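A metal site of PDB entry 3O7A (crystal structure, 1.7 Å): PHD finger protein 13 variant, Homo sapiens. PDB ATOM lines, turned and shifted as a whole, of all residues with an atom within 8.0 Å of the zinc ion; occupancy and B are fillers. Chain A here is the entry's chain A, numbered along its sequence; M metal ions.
The side-chain sulfur (SG) of Cys 24 sits close to the side-chain hydroxyl (OG1) of Thr 26.
N of Glu 23 lies close to SG of Cys 21.
The backbone NH (N) of Lys 48 lies close to the side-chain sulfur (SG) of Cys 46, 3.7 Å away.
N of Cys 21 is in hydrogen-bond range of O of Thr 26, at 2.8 Å.
Within 4 Å of the zinc ion: Cys 21, Cys 24, Cys 46 and Cys 49.
The nearest printed residue that does not touch the zinc ion is Glu 23 (4.7 Å).
The zinc ion is bound by SG of Cys 46, at 2.3 Å.
The side-chain sulfur (SG) of Cys 24 binds the zinc ion, 2.3 Å away.
SG of Cys 21 is bound to the zinc ion, at 2.3 Å.
The zinc ion is bound by SG of Cys 49 (2.3 Å).
The zinc ion has four donor atoms within binding distance.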
ATOM      1  N   PHE A   8     -25.004   5.264   8.042  1.00  0.00           N
ATOM      2  CA  PHE A   8     -25.891   5.260   9.207  1.00  0.00           C
ATOM      3  C   PHE A   8     -26.323   6.646   9.663  1.00  0.00           C
ATOM      4  O   PHE A   8     -27.238   6.774  10.442  1.00  0.00           O
ATOM      5  CB  PHE A   8     -25.250   4.485  10.386  1.00  0.00           C
ATOM      6  CG  PHE A   8     -23.860   4.879  10.659  1.00  0.00           C
ATOM      7  CD1 PHE A   8     -23.583   6.097  11.356  1.00  0.00           C
ATOM      8  CD2 PHE A   8     -22.784   4.064  10.242  1.00  0.00           C
ATOM      9  CE1 PHE A   8     -22.283   6.535  11.550  1.00  0.00           C
ATOM     10  CE2 PHE A   8     -21.451   4.476  10.519  1.00  0.00           C
ATOM     11  CZ  PHE A   8     -21.214   5.712  11.125  1.00  0.00           C
ATOM     12  N   GLU A  20     -16.287   1.677   2.026  1.00  0.00           N
ATOM     13  CA  GLU A  20     -17.232   0.571   2.111  1.00  0.00           C
ATOM     14  C   GLU A  20     -16.795  -0.322   3.250  1.00  0.00           C
ATOM     15  O   GLU A  20     -15.657  -0.810   3.264  1.00  0.00           O
ATOM     16  CB  GLU A  20     -17.270  -0.256   0.808  1.00  0.00           C
ATOM     17  CG  GLU A  20     -18.264  -1.376   0.853  1.00  0.00           C
ATOM     18  CD  GLU A  20     -18.013  -2.286  -0.352  1.00  0.00           C
ATOM     19  OE1 GLU A  20     -16.839  -2.359  -0.813  1.00  0.00           O
ATOM     20  OE2 GLU A  20     -18.941  -2.876  -0.844  1.00  0.00           O
ATOM     21  N   CYS A  21     -17.727  -0.615   4.154  1.00  0.00           N
ATOM     22  CA  CYS A  21     -17.435  -1.573   5.235  1.00  0.00           C
ATOM     23  C   CYS A  21     -17.095  -2.996   4.634  1.00  0.00           C
ATOM     24  O   CYS A  21     -17.821  -3.523   3.841  1.00  0.00           O
ATOM     25  CB  CYS A  21     -18.607  -1.627   6.227  1.00  0.00           C
ATOM     26  SG  CYS A  21     -18.319  -2.900   7.522  1.00  0.00           S
ATOM     27  N   ASN A  22     -15.975  -3.586   5.064  1.00  0.00           N
ATOM     28  CA  ASN A  22     -15.617  -4.929   4.599  1.00  0.00           C
ATOM     29  C   ASN A  22     -16.527  -6.076   5.121  1.00  0.00           C
ATOM     30  O   ASN A  22     -16.537  -7.190   4.578  1.00  0.00           O
ATOM     31  CB  ASN A  22     -14.143  -5.206   4.964  1.00  0.00           C
ATOM     32  CG  ASN A  22     -13.623  -6.435   4.319  1.00  0.00           C
ATOM     33  OD1 ASN A  22     -13.378  -7.437   5.001  1.00  0.00           O
ATOM     34  ND2 ASN A  22     -13.370  -6.368   3.007  1.00  0.00           N
ATOM     35  N   GLU A  23     -17.286  -5.829   6.201  1.00  0.00           N
ATOM     36  CA  GLU A  23     -18.187  -6.849   6.712  1.00  0.00           C
ATOM     37  C   GLU A  23     -19.666  -6.805   6.337  1.00  0.00           C
ATOM     38  O   GLU A  23     -20.305  -7.872   6.130  1.00  0.00           O
ATOM     39  CB  GLU A  23     -18.027  -6.969   8.211  1.00  0.00           C
ATOM     40  CG  GLU A  23     -16.744  -7.716   8.518  1.00  0.00           C
ATOM     41  CD  GLU A  23     -16.553  -7.961   9.982  1.00  0.00           C
ATOM     42  OE1 GLU A  23     -17.579  -8.092  10.722  1.00  0.00           O
ATOM     43  OE2 GLU A  23     -15.356  -8.008  10.391  1.00  0.00           O
ATOM     44  N   CYS A  24     -20.217  -5.596   6.240  1.00  0.00           N
ATOM     45  CA  CYS A  24     -21.597  -5.417   5.842  1.00  0.00           C
ATOM     46  C   CYS A  24     -21.754  -4.722   4.480  1.00  0.00           C
ATOM     47  O   CYS A  24     -22.872  -4.634   3.976  1.00  0.00           O
ATOM     48  CB  CYS A  24     -22.366  -4.599   6.875  1.00  0.00           C
ATOM     49  SG  CYS A  24     -21.957  -2.815   6.944  1.00  0.00           S
ATOM     50  N   HIS A  25     -20.630  -4.308   3.891  1.00  0.00           N
ATOM     51  CA  HIS A  25     -20.587  -3.770   2.507  1.00  0.00           C
ATOM     52  C   HIS A  25     -21.424  -2.529   2.341  1.00  0.00           C
ATOM     53  O   HIS A  25     -21.804  -2.189   1.239  1.00  0.00           O
ATOM     54  CB  HIS A  25     -20.915  -4.884   1.460  1.00  0.00           C
ATOM     55  CG  HIS A  25     -20.325  -6.202   1.826  1.00  0.00           C
ATOM     56  ND1 HIS A  25     -18.982  -6.468   1.698  1.00  0.00           N
ATOM     57  CD2 HIS A  25     -20.872  -7.274   2.454  1.00  0.00           C
ATOM     58  CE1 HIS A  25     -18.721  -7.664   2.230  1.00  0.00           C
ATOM     59  NE2 HIS A  25     -19.847  -8.163   2.698  1.00  0.00           N
ATOM     60  N   THR A  26     -21.592  -1.785   3.440  1.00  0.00           N
ATOM     61  CA  THR A  26     -22.292  -0.517   3.416  1.00  0.00           C
ATOM     62  C   THR A  26     -21.307   0.624   3.168  1.00  0.00           C
ATOM     63  O   THR A  26     -20.224   0.703   3.798  1.00  0.00           O
ATOM     64  CB  THR A  26     -23.008  -0.295   4.746  1.00  0.00           C
ATOM     65  OG1 THR A  26     -23.886  -1.425   4.964  1.00  0.00           O
ATOM     66  CG2 THR A  26     -23.868   1.005   4.713  1.00  0.00           C
ATOM     67  N   TRP A  27     -21.683   1.541   2.282  1.00  0.00           N
ATOM     68  CA  TRP A  27     -20.872   2.758   2.085  1.00  0.00           C
ATOM     69  C   TRP A  27     -21.130   3.752   3.244  1.00  0.00           C
ATOM     70  O   TRP A  27     -22.273   4.114   3.508  1.00  0.00           O
ATOM     71  CB  TRP A  27     -21.252   3.437   0.746  1.00  0.00           C
ATOM     72  CG  TRP A  27     -20.675   2.765  -0.446  1.00  0.00           C
ATOM     73  CD1 TRP A  27     -21.323   1.915  -1.341  1.00  0.00           C
ATOM     74  CD2 TRP A  27     -19.334   2.857  -0.886  1.00  0.00           C
ATOM     75  NE1 TRP A  27     -20.439   1.506  -2.308  1.00  0.00           N
ATOM     76  CE2 TRP A  27     -19.212   2.069  -2.055  1.00  0.00           C
ATOM     77  CE3 TRP A  27     -18.231   3.544  -0.416  1.00  0.00           C
ATOM     78  CZ2 TRP A  27     -18.022   1.995  -2.775  1.00  0.00           C
ATOM     79  CZ3 TRP A  27     -17.042   3.457  -1.133  1.00  0.00           C
ATOM     80  CH2 TRP A  27     -16.937   2.652  -2.281  1.00  0.00           C
ATOM     81  N   ILE A  28     -20.053   4.170   3.900  1.00  0.00           N
ATOM     82  CA  ILE A  28     -20.099   5.060   5.052  1.00  0.00           C
ATOM     83  C   ILE A  28     -19.274   6.299   4.762  1.00  0.00           C
ATOM     84  O   ILE A  28     -18.218   6.229   4.136  1.00  0.00           O
ATOM     85  CB  ILE A  28     -19.419   4.319   6.293  1.00  0.00           C
ATOM     86  CG1 ILE A  28     -20.069   2.941   6.538  1.00  0.00           C
ATOM     87  CG2 ILE A  28     -19.360   5.211   7.534  1.00  0.00           C
ATOM     88  CD1 ILE A  28     -21.498   3.028   6.853  1.00  0.00           C
ATOM     89  N   PHE A  44     -11.539  -1.730   6.345  1.00  0.00           N
ATOM     90  CA  PHE A  44     -12.434  -0.894   7.120  1.00  0.00           C
ATOM     91  C   PHE A  44     -13.601  -1.730   7.597  1.00  0.00           C
ATOM     92  O   PHE A  44     -14.201  -2.464   6.810  1.00  0.00           O
ATOM     93  CB  PHE A  44     -13.004   0.240   6.259  1.00  0.00           C
ATOM     94  CG  PHE A  44     -14.105   0.991   6.940  1.00  0.00           C
ATOM     95  CD1 PHE A  44     -13.865   1.647   8.161  1.00  0.00           C
ATOM     96  CD2 PHE A  44     -15.381   1.021   6.377  1.00  0.00           C
ATOM     97  CE1 PHE A  44     -14.915   2.292   8.864  1.00  0.00           C
ATOM     98  CE2 PHE A  44     -16.458   1.679   7.066  1.00  0.00           C
ATOM     99  CZ  PHE A  44     -16.216   2.326   8.283  1.00  0.00           C
ATOM    100  N   VAL A  45     -13.846  -1.697   8.904  1.00  0.00           N
ATOM    101  CA  VAL A  45     -15.032  -2.300   9.482  1.00  0.00           C
ATOM    102  C   VAL A  45     -15.822  -1.214  10.286  1.00  0.00           C
ATOM    103  O   VAL A  45     -15.250  -0.543  11.209  1.00  0.00           O
ATOM    104  CB  VAL A  45     -14.695  -3.507  10.398  1.00  0.00           C
ATOM    105  CG1 VAL A  45     -16.006  -4.060  11.015  1.00  0.00           C
ATOM    106  CG2 VAL A  45     -13.976  -4.548   9.523  1.00  0.00           C
ATOM    107  N   CYS A  46     -17.108  -1.045   9.952  1.00  0.00           N
ATOM    108  CA  CYS A  46     -17.880   0.075  10.458  1.00  0.00           C
ATOM    109  C   CYS A  46     -18.270  -0.164  11.920  1.00  0.00           C
ATOM    110  O   CYS A  46     -18.203  -1.294  12.389  1.00  0.00           O
ATOM    111  CB  CYS A  46     -19.140   0.302   9.582  1.00  0.00           C
ATOM    112  SG  CYS A  46     -20.508  -0.830   9.900  1.00  0.00           S
ATOM    113  N   GLN A  47     -18.678   0.896  12.604  1.00  0.00           N
ATOM    114  CA  GLN A  47     -18.980   0.844  14.010  1.00  0.00           C
ATOM    115  C   GLN A  47     -20.123  -0.107  14.305  1.00  0.00           C
ATOM    116  O   GLN A  47     -20.062  -0.860  15.290  1.00  0.00           O
ATOM    117  CB  GLN A  47     -19.308   2.252  14.580  1.00  0.00           C
ATOM    118  CG  GLN A  47     -19.549   2.251  16.155  1.00  0.00           C
ATOM    119  CD  GLN A  47     -18.260   1.997  16.986  1.00  0.00           C
ATOM    120  OE1 GLN A  47     -17.392   2.877  17.073  1.00  0.00           O
ATOM    121  NE2 GLN A  47     -18.158   0.810  17.592  1.00  0.00           N
ATOM    122  N   LYS A  48     -21.133  -0.122  13.455  1.00  0.00           N
ATOM    123  CA  LYS A  48     -22.259  -1.058  13.652  1.00  0.00           C
ATOM    124  C   LYS A  48     -21.817  -2.498  13.643  1.00  0.00           C
ATOM    125  O   LYS A  48     -22.315  -3.323  14.443  1.00  0.00           O
ATOM    126  CB  LYS A  48     -23.391  -0.816  12.668  1.00  0.00           C
ATOM    127  CG  LYS A  48     -24.062   0.572  12.799  1.00  0.00           C
ATOM    128  CD  LYS A  48     -25.592   0.524  12.622  1.00  0.00           C
ATOM    129  CE  LYS A  48     -26.039   0.832  11.172  1.00  0.00           C
ATOM    130  NZ  LYS A  48     -27.332   1.604  11.105  1.00  0.00           N
ATOM    131  N   CYS A  49     -20.882  -2.818  12.754  1.00  0.00           N
ATOM    132  CA  CYS A  49     -20.377  -4.178  12.657  1.00  0.00           C
ATOM    133  C   CYS A  49     -19.508  -4.515  13.886  1.00  0.00           C
ATOM    134  O   CYS A  49     -19.633  -5.615  14.457  1.00  0.00           O
ATOM    135  CB  CYS A  49     -19.603  -4.385  11.371  1.00  0.00           C
ATOM    136  SG  CYS A  49     -20.714  -4.638   9.959  1.00  0.00           S
ATOM    137  N   ARG A  50     -18.685  -3.562  14.296  1.00  0.00           N
ATOM    138  CA  ARG A  50     -17.841  -3.692  15.505  1.00  0.00           C
ATOM    139  C   ARG A  50     -18.632  -3.882  16.832  1.00  0.00           C
ATOM    140  O   ARG A  50     -18.106  -4.491  17.791  1.00  0.00           O
ATOM    141  CB  ARG A  50     -16.886  -2.489  15.628  1.00  0.00           C
ATOM    142  CG  ARG A  50     -15.686  -2.541  14.688  1.00  0.00           C
ATOM    143  CD  ARG A  50     -14.580  -3.435  15.247  1.00  0.00           C
ATOM    144  NE  ARG A  50     -13.593  -2.658  16.000  1.00  0.00           N
ATOM    145  CZ  ARG A  50     -12.921  -3.072  17.082  1.00  0.00           C
ATOM    146  NH1 ARG A  50     -13.112  -4.285  17.591  1.00  0.00           N
ATOM    147  NH2 ARG A  50     -12.035  -2.252  17.651  1.00  0.00           N
ATOM    148  N   SER A  52     -21.062  -5.768  17.267  1.00  0.00           N
ATOM    149  CA  SER A  52     -21.778  -7.067  17.013  1.00  0.00           C
ATOM    150  C   SER A  52     -23.084  -6.910  16.237  1.00  0.00           C
ATOM    151  O   SER A  52     -23.079  -6.440  15.095  1.00  0.00           O
ATOM    152  CB  SER A  52     -21.985  -7.895  18.306  1.00  0.00           C
HETATM  153 ZN    ZN M   1     -20.365  -2.743   8.633  1.00  0.00          ZN
